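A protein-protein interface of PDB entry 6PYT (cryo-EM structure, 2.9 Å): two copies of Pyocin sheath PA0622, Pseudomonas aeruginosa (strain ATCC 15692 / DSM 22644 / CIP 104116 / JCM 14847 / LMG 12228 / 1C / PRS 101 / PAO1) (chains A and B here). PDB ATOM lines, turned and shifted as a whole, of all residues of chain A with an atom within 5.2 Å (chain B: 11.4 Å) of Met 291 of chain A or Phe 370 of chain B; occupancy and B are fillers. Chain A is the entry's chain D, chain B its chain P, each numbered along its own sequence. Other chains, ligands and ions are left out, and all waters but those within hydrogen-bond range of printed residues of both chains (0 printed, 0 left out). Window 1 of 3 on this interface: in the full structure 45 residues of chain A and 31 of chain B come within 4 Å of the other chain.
O of Asn 369 of chain B sits at hydrogen-bond distance from N of Trp 355 of chain A, 2.8 Å away.
The backbone NH (N) of Arg 371 of chain B sits at hydrogen-bond distance from the backbone carbonyl oxygen (O) of Trp 355 of chain A.
The backbone carbonyl oxygen (O) of Arg 371 of chain B sits at hydrogen-bond distance from the backbone NH (N) of Ile 357 of chain A (2.9 Å).
The side-chain amide oxygen (OD1) of Asn 369 of chain B sits close to the side-chain amide oxygen (OD1) of Asn 367 of chain B (3.2 Å).
Among the printed residues, merely in contact across the chains: Met 287 of chain A with Val 372 of chain B, Met 287 of chain A with Val 374 of chain B, Met 291 of chain A with Phe 370 of chain B, Met 291 of chain A with Val 372 of chain B, Ile 294 of chain A with Phe 370 of chain B, Leu 295 of chain A with Phe 370 of chain B, Leu 318 of chain A with Phe 370 of chain B, Trp 355 of chain A with Pro 368 of chain B, Trp 355 of chain A with Phe 370 of chain B, Ile 357 of chain A with Phe 370 of chain B, Ile 357 of chain A with Val 372 of chain B and Ile 357 of chain A with Glu 373 of chain B.
Met 287 of chain A touches two residues of chain B.
Met 291 of chain A touches just these residues of chain B: Phe 370 and Val 372.
No residue of chain B comes within 4 Å of Asp 292 of chain A.
No residue of chain B comes within 4 Å of Ala 293 of chain A.
No residue of chain B comes within 4 Å of His 298 of chain A.
Printed residues of chain B within 4 Å of Leu 318 of chain A: Phe 370.
Trp 355 of chain A touches four residues of chain B.
Of chain B, only Phe 370, Arg 371, Val 372 and Glu 373 come within 4 Å of Ile 357 of chain A.
Of the printed residues of chain A, Pro 368 of chain B touches Trp 355.
Of the printed residues of chain A, Asn 369 of chain B touches Trp 355.
Of chain A, only Met 291 (3.9 Å), Ile 294 (3.7 Å), Leu 295 (3.7 Å), Leu 318 (3.7 Å), Trp 355 (3.5 Å) and Ile 357 (3.5 Å) come within 4 Å of Phe 370 of chain B.
Of the printed residues of chain A, Arg 371 of chain B touches Trp 355 and Ile 357.
Printed residues of chain A within 4 Å of Val 374 of chain B: Met 287.
The nearest residue of chain B that does not touch Met 291 of chain A is Arg 371 of chain B (6.4 Å).
The nearest residue of chain A that does not touch Phe 370 of chain B is Val 314 of chain A (4.3 Å).
The nearest printed residue of chain A that does not touch Arg 371 of chain B is Met 291 of chain A (6.4 Å).
Of the 16 printed residues of chain A, 7 touch a printed residue of chain B.
Along chain A the printed residues that touch a printed residue of chain B span positions 287 to 357.
Among the printed residues, no Asp or Glu carboxylate lies within 4 Å of a Lys or Arg side-chain nitrogen of the other chain.
No position is printed for both chains.
Of the 15 pairs that touch across the chains among the printed residues, none has its exchanged pair printed and touching as well.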
ATOM      1  N   THR A 286      -9.439 -29.709 -36.375  1.00  0.00           N
ATOM      2  CA  THR A 286     -10.147 -30.307 -35.245  1.00  0.00           C
ATOM      3  C   THR A 286      -9.343 -30.166 -33.969  1.00  0.00           C
ATOM      4  O   THR A 286      -9.874 -29.734 -32.944  1.00  0.00           O
ATOM      5  CB  THR A 286     -10.446 -31.780 -35.504  1.00  0.00           C
ATOM      6  OG1 THR A 286     -11.228 -31.906 -36.693  1.00  0.00           O
ATOM      7  CG2 THR A 286     -11.199 -32.399 -34.348  1.00  0.00           C
ATOM      8  N   MET A 287      -8.051 -30.505 -34.026  1.00  0.00           N
ATOM      9  CA  MET A 287      -7.160 -30.358 -32.879  1.00  0.00           C
ATOM     10  C   MET A 287      -7.029 -28.904 -32.458  1.00  0.00           C
ATOM     11  O   MET A 287      -6.861 -28.611 -31.271  1.00  0.00           O
ATOM     12  CB  MET A 287      -5.790 -30.953 -33.222  1.00  0.00           C
ATOM     13  CG  MET A 287      -4.739 -30.934 -32.116  1.00  0.00           C
ATOM     14  SD  MET A 287      -3.688 -29.471 -32.108  1.00  0.00           S
ATOM     15  CE  MET A 287      -2.769 -29.710 -30.598  1.00  0.00           C
ATOM     16  N   ASP A 288      -7.131 -27.984 -33.411  1.00  0.00           N
ATOM     17  CA  ASP A 288      -7.049 -26.566 -33.096  1.00  0.00           C
ATOM     18  C   ASP A 288      -8.322 -26.069 -32.430  1.00  0.00           C
ATOM     19  O   ASP A 288      -8.264 -25.251 -31.508  1.00  0.00           O
ATOM     20  CB  ASP A 288      -6.778 -25.773 -34.369  1.00  0.00           C
ATOM     21  N   LEU A 289      -9.478 -26.541 -32.880  1.00  0.00           N
ATOM     22  CA  LEU A 289     -10.746 -26.064 -32.353  1.00  0.00           C
ATOM     23  C   LEU A 289     -11.419 -27.033 -31.393  1.00  0.00           C
ATOM     24  O   LEU A 289     -12.515 -26.737 -30.915  1.00  0.00           O
ATOM     25  CB  LEU A 289     -11.700 -25.724 -33.495  1.00  0.00           C
ATOM     26  CG  LEU A 289     -11.308 -24.493 -34.302  1.00  0.00           C
ATOM     27  CD1 LEU A 289     -12.185 -24.355 -35.500  1.00  0.00           C
ATOM     28  CD2 LEU A 289     -11.430 -23.260 -33.444  1.00  0.00           C
ATOM     29  N   VAL A 290     -10.805 -28.178 -31.090  1.00  0.00           N
ATOM     30  CA  VAL A 290     -11.231 -28.883 -29.891  1.00  0.00           C
ATOM     31  C   VAL A 290     -10.700 -28.148 -28.675  1.00  0.00           C
ATOM     32  O   VAL A 290     -11.358 -28.102 -27.632  1.00  0.00           O
ATOM     33  CB  VAL A 290     -10.805 -30.368 -29.915  1.00  0.00           C
ATOM     34  CG1 VAL A 290      -9.302 -30.549 -29.836  1.00  0.00           C
ATOM     35  CG2 VAL A 290     -11.438 -31.122 -28.816  1.00  0.00           C
ATOM     36  N   MET A 291      -9.547 -27.494 -28.800  1.00  0.00           N
ATOM     37  CA  MET A 291      -8.963 -26.875 -27.630  1.00  0.00           C
ATOM     38  C   MET A 291      -9.546 -25.502 -27.395  1.00  0.00           C
ATOM     39  O   MET A 291      -9.774 -25.127 -26.246  1.00  0.00           O
ATOM     40  CB  MET A 291      -7.447 -26.815 -27.764  1.00  0.00           C
ATOM     41  CG  MET A 291      -6.847 -28.188 -27.933  1.00  0.00           C
ATOM     42  SD  MET A 291      -7.477 -29.380 -26.736  1.00  0.00           S
ATOM     43  CE  MET A 291      -6.844 -28.746 -25.191  1.00  0.00           C
ATOM     44  N   ASP A 292      -9.854 -24.776 -28.466  1.00  0.00           N
ATOM     45  CA  ASP A 292     -10.494 -23.477 -28.330  1.00  0.00           C
ATOM     46  C   ASP A 292     -11.895 -23.576 -27.747  1.00  0.00           C
ATOM     47  O   ASP A 292     -12.386 -22.593 -27.192  1.00  0.00           O
ATOM     48  CB  ASP A 292     -10.539 -22.783 -29.685  1.00  0.00           C
ATOM     49  N   ALA A 293     -12.548 -24.730 -27.863  1.00  0.00           N
ATOM     50  CA  ALA A 293     -13.776 -24.962 -27.115  1.00  0.00           C
ATOM     51  C   ALA A 293     -13.473 -25.426 -25.697  1.00  0.00           C
ATOM     52  O   ALA A 293     -14.207 -25.087 -24.764  1.00  0.00           O
ATOM     53  CB  ALA A 293     -14.647 -25.985 -27.838  1.00  0.00           C
ATOM     54  N   ILE A 294     -12.394 -26.189 -25.523  1.00  0.00           N
ATOM     55  CA  ILE A 294     -11.954 -26.600 -24.193  1.00  0.00           C
ATOM     56  C   ILE A 294     -11.465 -25.404 -23.388  1.00  0.00           C
ATOM     57  O   ILE A 294     -11.826 -25.245 -22.216  1.00  0.00           O
ATOM     58  CB  ILE A 294     -10.885 -27.703 -24.304  1.00  0.00           C
ATOM     59  CG1 ILE A 294     -11.552 -29.051 -24.555  1.00  0.00           C
ATOM     60  CG2 ILE A 294      -9.958 -27.742 -23.104  1.00  0.00           C
ATOM     61  CD1 ILE A 294     -12.451 -29.475 -23.432  1.00  0.00           C
ATOM     62  N   LEU A 295     -10.661 -24.535 -24.003  1.00  0.00           N
ATOM     63  CA  LEU A 295     -10.131 -23.388 -23.269  1.00  0.00           C
ATOM     64  C   LEU A 295     -11.223 -22.370 -22.983  1.00  0.00           C
ATOM     65  O   LEU A 295     -11.438 -21.990 -21.830  1.00  0.00           O
ATOM     66  CB  LEU A 295      -8.984 -22.736 -24.036  1.00  0.00           C
ATOM     67  CG  LEU A 295      -7.749 -23.599 -24.301  1.00  0.00           C
ATOM     68  CD1 LEU A 295      -6.663 -22.825 -25.018  1.00  0.00           C
ATOM     69  CD2 LEU A 295      -7.249 -24.270 -23.059  1.00  0.00           C
ATOM     70  N   ALA A 296     -11.933 -21.926 -24.013  1.00  0.00           N
ATOM     71  CA  ALA A 296     -13.052 -21.009 -23.815  1.00  0.00           C
ATOM     72  C   ALA A 296     -14.214 -21.831 -23.284  1.00  0.00           C
ATOM     73  O   ALA A 296     -15.059 -22.321 -24.033  1.00  0.00           O
ATOM     74  CB  ALA A 296     -13.406 -20.284 -25.105  1.00  0.00           C
ATOM     75  N   HIS A 298     -13.197 -23.297 -19.964  1.00  0.00           N
ATOM     76  CA  HIS A 298     -12.449 -23.551 -18.741  1.00  0.00           C
ATOM     77  C   HIS A 298     -11.550 -22.374 -18.431  1.00  0.00           C
ATOM     78  O   HIS A 298     -10.354 -22.512 -18.177  1.00  0.00           O
ATOM     79  CB  HIS A 298     -11.648 -24.838 -18.820  1.00  0.00           C
ATOM     80  CG  HIS A 298     -12.505 -26.058 -18.854  1.00  0.00           C
ATOM     81  ND1 HIS A 298     -13.265 -26.452 -17.776  1.00  0.00           N
ATOM     82  CD2 HIS A 298     -12.715 -26.980 -19.821  1.00  0.00           C
ATOM     83  CE1 HIS A 298     -13.921 -27.554 -18.086  1.00  0.00           C
ATOM     84  NE2 HIS A 298     -13.602 -27.897 -19.320  1.00  0.00           N
ATOM     85  N   VAL A 314     -11.372 -30.372 -12.697  1.00  0.00           N
ATOM     86  CA  VAL A 314     -11.019 -30.027 -14.066  1.00  0.00           C
ATOM     87  C   VAL A 314     -11.218 -31.221 -14.990  1.00  0.00           C
ATOM     88  O   VAL A 314     -11.764 -31.062 -16.086  1.00  0.00           O
ATOM     89  CB  VAL A 314      -9.587 -29.469 -14.126  1.00  0.00           C
ATOM     90  CG1 VAL A 314      -9.141 -29.269 -15.551  1.00  0.00           C
ATOM     91  CG2 VAL A 314      -9.520 -28.144 -13.412  1.00  0.00           C
ATOM     92  N   LEU A 318     -13.326 -31.306 -17.975  1.00  0.00           N
ATOM     93  CA  LEU A 318     -12.778 -31.574 -19.298  1.00  0.00           C
ATOM     94  C   LEU A 318     -13.516 -32.707 -19.985  1.00  0.00           C
ATOM     95  O   LEU A 318     -13.756 -32.639 -21.188  1.00  0.00           O
ATOM     96  CB  LEU A 318     -11.291 -31.900 -19.223  1.00  0.00           C
ATOM     97  CG  LEU A 318     -10.303 -30.778 -18.967  1.00  0.00           C
ATOM     98  CD1 LEU A 318      -8.929 -31.352 -18.753  1.00  0.00           C
ATOM     99  CD2 LEU A 318     -10.322 -29.887 -20.147  1.00  0.00           C
ATOM    100  N   TRP A 355      -2.565 -32.361 -17.477  1.00  0.00           N
ATOM    101  CA  TRP A 355      -3.640 -33.252 -17.891  1.00  0.00           C
ATOM    102  C   TRP A 355      -3.332 -33.804 -19.273  1.00  0.00           C
ATOM    103  O   TRP A 355      -2.579 -33.209 -20.040  1.00  0.00           O
ATOM    104  CB  TRP A 355      -4.991 -32.541 -17.913  1.00  0.00           C
ATOM    105  CG  TRP A 355      -5.503 -32.210 -16.568  1.00  0.00           C
ATOM    106  CD1 TRP A 355      -6.199 -33.025 -15.753  1.00  0.00           C
ATOM    107  CD2 TRP A 355      -5.388 -30.963 -15.886  1.00  0.00           C
ATOM    108  NE1 TRP A 355      -6.516 -32.382 -14.592  1.00  0.00           N
ATOM    109  CE2 TRP A 355      -6.029 -31.108 -14.650  1.00  0.00           C
ATOM    110  CE3 TRP A 355      -4.795 -29.742 -16.195  1.00  0.00           C
ATOM    111  CZ2 TRP A 355      -6.098 -30.086 -13.727  1.00  0.00           C
ATOM    112  CZ3 TRP A 355      -4.872 -28.727 -15.282  1.00  0.00           C
ATOM    113  CH2 TRP A 355      -5.521 -28.901 -14.064  1.00  0.00           C
ATOM    114  N   ILE A 357      -5.152 -35.305 -22.782  1.00  0.00           N
ATOM    115  CA  ILE A 357      -6.432 -35.140 -23.475  1.00  0.00           C
ATOM    116  C   ILE A 357      -6.406 -35.854 -24.829  1.00  0.00           C
ATOM    117  O   ILE A 357      -6.656 -35.232 -25.866  1.00  0.00           O
ATOM    118  CB  ILE A 357      -6.819 -33.652 -23.623  1.00  0.00           C
ATOM    119  CG1 ILE A 357      -6.631 -32.901 -22.315  1.00  0.00           C
ATOM    120  CG2 ILE A 357      -8.318 -33.507 -23.827  1.00  0.00           C
ATOM    121  CD1 ILE A 357      -6.775 -31.423 -22.448  1.00  0.00           C
ATOM    122  N   ASN B 223      -7.927 -13.380 -12.772  1.00  0.00           N
ATOM    123  CA  ASN B 223      -8.719 -13.759 -13.929  1.00  0.00           C
ATOM    124  C   ASN B 223     -10.086 -13.103 -13.862  1.00  0.00           C
ATOM    125  O   ASN B 223     -10.970 -13.451 -14.651  1.00  0.00           O
ATOM    126  CB  ASN B 223      -8.834 -15.279 -14.014  1.00  0.00           C
ATOM    127  CG  ASN B 223      -9.116 -15.768 -15.407  1.00  0.00           C
ATOM    128  OD1 ASN B 223      -9.211 -14.983 -16.339  1.00  0.00           O
ATOM    129  ND2 ASN B 223      -9.239 -17.074 -15.560  1.00  0.00           N
ATOM    130  N   PHE B 238      -2.571 -12.635 -25.405  1.00  0.00           N
ATOM    131  CA  PHE B 238      -2.323 -13.901 -24.734  1.00  0.00           C
ATOM    132  C   PHE B 238      -2.496 -15.050 -25.711  1.00  0.00           C
ATOM    133  O   PHE B 238      -3.620 -15.414 -26.066  1.00  0.00           O
ATOM    134  CB  PHE B 238      -3.196 -14.132 -23.513  1.00  0.00           C
ATOM    135  CG  PHE B 238      -2.989 -15.491 -22.942  1.00  0.00           C
ATOM    136  CD1 PHE B 238      -1.755 -15.841 -22.423  1.00  0.00           C
ATOM    137  CD2 PHE B 238      -3.999 -16.437 -22.961  1.00  0.00           C
ATOM    138  CE1 PHE B 238      -1.535 -17.100 -21.922  1.00  0.00           C
ATOM    139  CE2 PHE B 238      -3.782 -17.703 -22.454  1.00  0.00           C
ATOM    140  CZ  PHE B 238      -2.547 -18.032 -21.933  1.00  0.00           C
ATOM    141  N   ASP B 240      -0.186 -18.947 -27.019  1.00  0.00           N
ATOM    142  CA  ASP B 240       0.654 -20.013 -26.487  1.00  0.00           C
ATOM    143  C   ASP B 240       1.821 -20.270 -27.438  1.00  0.00           C
ATOM    144  O   ASP B 240       2.037 -19.534 -28.403  1.00  0.00           O
ATOM    145  CB  ASP B 240      -0.170 -21.278 -26.264  1.00  0.00           C
ATOM    146  N   GLY B 241       2.582 -21.316 -27.151  1.00  0.00           N
ATOM    147  CA  GLY B 241       3.584 -21.813 -28.064  1.00  0.00           C
ATOM    148  C   GLY B 241       5.013 -21.396 -27.797  1.00  0.00           C
ATOM    149  O   GLY B 241       5.807 -21.381 -28.747  1.00  0.00           O
ATOM    150  N   TRP B 267      -4.964  -9.913 -15.549  1.00  0.00           N
ATOM    151  CA  TRP B 267      -4.364 -11.172 -15.958  1.00  0.00           C
ATOM    152  C   TRP B 267      -3.239 -11.664 -15.065  1.00  0.00           C
ATOM    153  O   TRP B 267      -3.284 -12.815 -14.632  1.00  0.00           O
ATOM    154  CB  TRP B 267      -3.913 -11.059 -17.416  1.00  0.00           C
ATOM    155  CG  TRP B 267      -3.406 -12.325 -18.025  1.00  0.00           C
ATOM    156  CD1 TRP B 267      -2.176 -12.529 -18.555  1.00  0.00           C
ATOM    157  CD2 TRP B 267      -4.102 -13.574 -18.139  1.00  0.00           C
ATOM    158  NE1 TRP B 267      -2.067 -13.807 -19.023  1.00  0.00           N
ATOM    159  CE2 TRP B 267      -3.236 -14.470 -18.774  1.00  0.00           C
ATOM    160  CE3 TRP B 267      -5.380 -14.017 -17.779  1.00  0.00           C
ATOM    161  CZ2 TRP B 267      -3.593 -15.772 -19.050  1.00  0.00           C
ATOM    162  CZ3 TRP B 267      -5.727 -15.310 -18.048  1.00  0.00           C
ATOM    163  CH2 TRP B 267      -4.841 -16.175 -18.678  1.00  0.00           C
ATOM    164  N   ALA B 365      -3.717 -21.455  -9.064  1.00  0.00           N
ATOM    165  CA  ALA B 365      -3.562 -22.351 -10.208  1.00  0.00           C
ATOM    166  C   ALA B 365      -3.071 -21.539 -11.401  1.00  0.00           C
ATOM    167  O   ALA B 365      -3.814 -21.226 -12.330  1.00  0.00           O
ATOM    168  CB  ALA B 365      -4.874 -23.059 -10.515  1.00  0.00           C
ATOM    169  N   GLU B 366      -1.775 -21.224 -11.378  1.00  0.00           N
ATOM    170  CA  GLU B 366      -1.220 -20.241 -12.304  1.00  0.00           C
ATOM    171  C   GLU B 366      -1.121 -20.791 -13.718  1.00  0.00           C
ATOM    172  O   GLU B 366      -1.347 -20.063 -14.688  1.00  0.00           O
ATOM    173  CB  GLU B 366       0.160 -19.799 -11.824  1.00  0.00           C
ATOM    174  N   ASN B 367      -0.798 -22.071 -13.860  1.00  0.00           N
ATOM    175  CA  ASN B 367      -0.491 -22.662 -15.161  1.00  0.00           C
ATOM    176  C   ASN B 367      -1.093 -24.053 -15.273  1.00  0.00           C
ATOM    177  O   ASN B 367      -0.415 -25.058 -15.045  1.00  0.00           O
ATOM    178  CB  ASN B 367       1.022 -22.717 -15.371  1.00  0.00           C
ATOM    179  CG  ASN B 367       1.410 -23.024 -16.791  1.00  0.00           C
ATOM    180  OD1 ASN B 367       0.576 -23.082 -17.682  1.00  0.00           O
ATOM    181  ND2 ASN B 367       2.693 -23.253 -17.005  1.00  0.00           N
ATOM    182  N   PRO B 368      -2.364 -24.158 -15.653  1.00  0.00           N
ATOM    183  CA  PRO B 368      -2.898 -25.474 -16.012  1.00  0.00           C
ATOM    184  C   PRO B 368      -2.348 -25.922 -17.354  1.00  0.00           C
ATOM    185  O   PRO B 368      -2.264 -25.143 -18.301  1.00  0.00           O
ATOM    186  CB  PRO B 368      -4.407 -25.241 -16.064  1.00  0.00           C
ATOM    187  CG  PRO B 368      -4.552 -23.820 -16.343  1.00  0.00           C
ATOM    188  CD  PRO B 368      -3.411 -23.126 -15.676  1.00  0.00           C
ATOM    189  N   ASN B 369      -1.945 -27.184 -17.426  1.00  0.00           N
ATOM    190  CA  ASN B 369      -1.239 -27.701 -18.589  1.00  0.00           C
ATOM    191  C   ASN B 369      -2.035 -28.832 -19.211  1.00  0.00           C
ATOM    192  O   ASN B 369      -2.338 -29.825 -18.546  1.00  0.00           O
ATOM    193  CB  ASN B 369       0.164 -28.161 -18.209  1.00  0.00           C
ATOM    194  CG  ASN B 369       1.090 -27.007 -17.964  1.00  0.00           C
ATOM    195  OD1 ASN B 369       1.108 -26.051 -18.726  1.00  0.00           O
ATOM    196  ND2 ASN B 369       1.852 -27.073 -16.894  1.00  0.00           N
ATOM    197  N   PHE B 370      -2.368 -28.681 -20.484  1.00  0.00           N
ATOM    198  CA  PHE B 370      -3.142 -29.661 -21.227  1.00  0.00           C
ATOM    199  C   PHE B 370      -2.221 -30.347 -22.222  1.00  0.00           C
ATOM    200  O   PHE B 370      -1.646 -29.689 -23.089  1.00  0.00           O
ATOM    201  CB  PHE B 370      -4.304 -28.990 -21.950  1.00  0.00           C
ATOM    202  CG  PHE B 370      -5.393 -28.508 -21.044  1.00  0.00           C
ATOM    203  CD1 PHE B 370      -5.519 -28.991 -19.756  1.00  0.00           C
ATOM    204  CD2 PHE B 370      -6.291 -27.557 -21.482  1.00  0.00           C
ATOM    205  CE1 PHE B 370      -6.524 -28.541 -18.932  1.00  0.00           C
ATOM    206  CE2 PHE B 370      -7.299 -27.106 -20.653  1.00  0.00           C
ATOM    207  CZ  PHE B 370      -7.407 -27.600 -19.378  1.00  0.00           C
ATOM    208  N   ARG B 371      -2.072 -31.659 -22.094  1.00  0.00           N
ATOM    209  CA  ARG B 371      -1.211 -32.436 -22.980  1.00  0.00           C
ATOM    210  C   ARG B 371      -2.126 -33.209 -23.920  1.00  0.00           C
ATOM    211  O   ARG B 371      -2.540 -34.328 -23.634  1.00  0.00           O
ATOM    212  CB  ARG B 371      -0.313 -33.367 -22.186  1.00  0.00           C
ATOM    213  CG  ARG B 371       0.586 -32.683 -21.199  1.00  0.00           C
ATOM    214  CD  ARG B 371       1.332 -33.729 -20.426  1.00  0.00           C
ATOM    215  NE  ARG B 371       2.275 -34.427 -21.285  1.00  0.00           N
ATOM    216  CZ  ARG B 371       2.844 -35.585 -20.984  1.00  0.00           C
ATOM    217  NH1 ARG B 371       2.543 -36.198 -19.852  1.00  0.00           N
ATOM    218  NH2 ARG B 371       3.698 -36.139 -21.826  1.00  0.00           N
ATOM    219  N   VAL B 372      -2.433 -32.606 -25.049  1.00  0.00           N
ATOM    220  CA  VAL B 372      -3.450 -33.106 -25.962  1.00  0.00           C
ATOM    221  C   VAL B 372      -2.779 -33.869 -27.098  1.00  0.00           C
ATOM    222  O   VAL B 372      -1.705 -33.488 -27.570  1.00  0.00           O
ATOM    223  CB  VAL B 372      -4.326 -31.933 -26.450  1.00  0.00           C
ATOM    224  CG1 VAL B 372      -3.483 -30.838 -27.058  1.00  0.00           C
ATOM    225  CG2 VAL B 372      -5.394 -32.382 -27.417  1.00  0.00           C
ATOM    226  N   GLU B 373      -3.387 -34.985 -27.500  1.00  0.00           N
ATOM    227  CA  GLU B 373      -2.845 -35.869 -28.519  1.00  0.00           C
ATOM    228  C   GLU B 373      -3.966 -36.370 -29.413  1.00  0.00           C
ATOM    229  O   GLU B 373      -5.030 -36.751 -28.925  1.00  0.00           O
ATOM    230  CB  GLU B 373      -2.146 -37.066 -27.883  1.00  0.00           C
ATOM    231  N   VAL B 374      -3.723 -36.385 -30.717  1.00  0.00           N
ATOM    232  CA  VAL B 374      -4.639 -36.985 -31.673  1.00  0.00           C
ATOM    233  C   VAL B 374      -4.135 -38.385 -31.988  1.00  0.00           C
ATOM    234  O   VAL B 374      -3.012 -38.553 -32.478  1.00  0.00           O
ATOM    235  CB  VAL B 374      -4.745 -36.150 -32.953  1.00  0.00           C
ATOM    236  CG1 VAL B 374      -5.721 -36.792 -33.871  1.00  0.00           C
ATOM    237  CG2 VAL B 374      -5.174 -34.751 -32.639  1.00  0.00           C
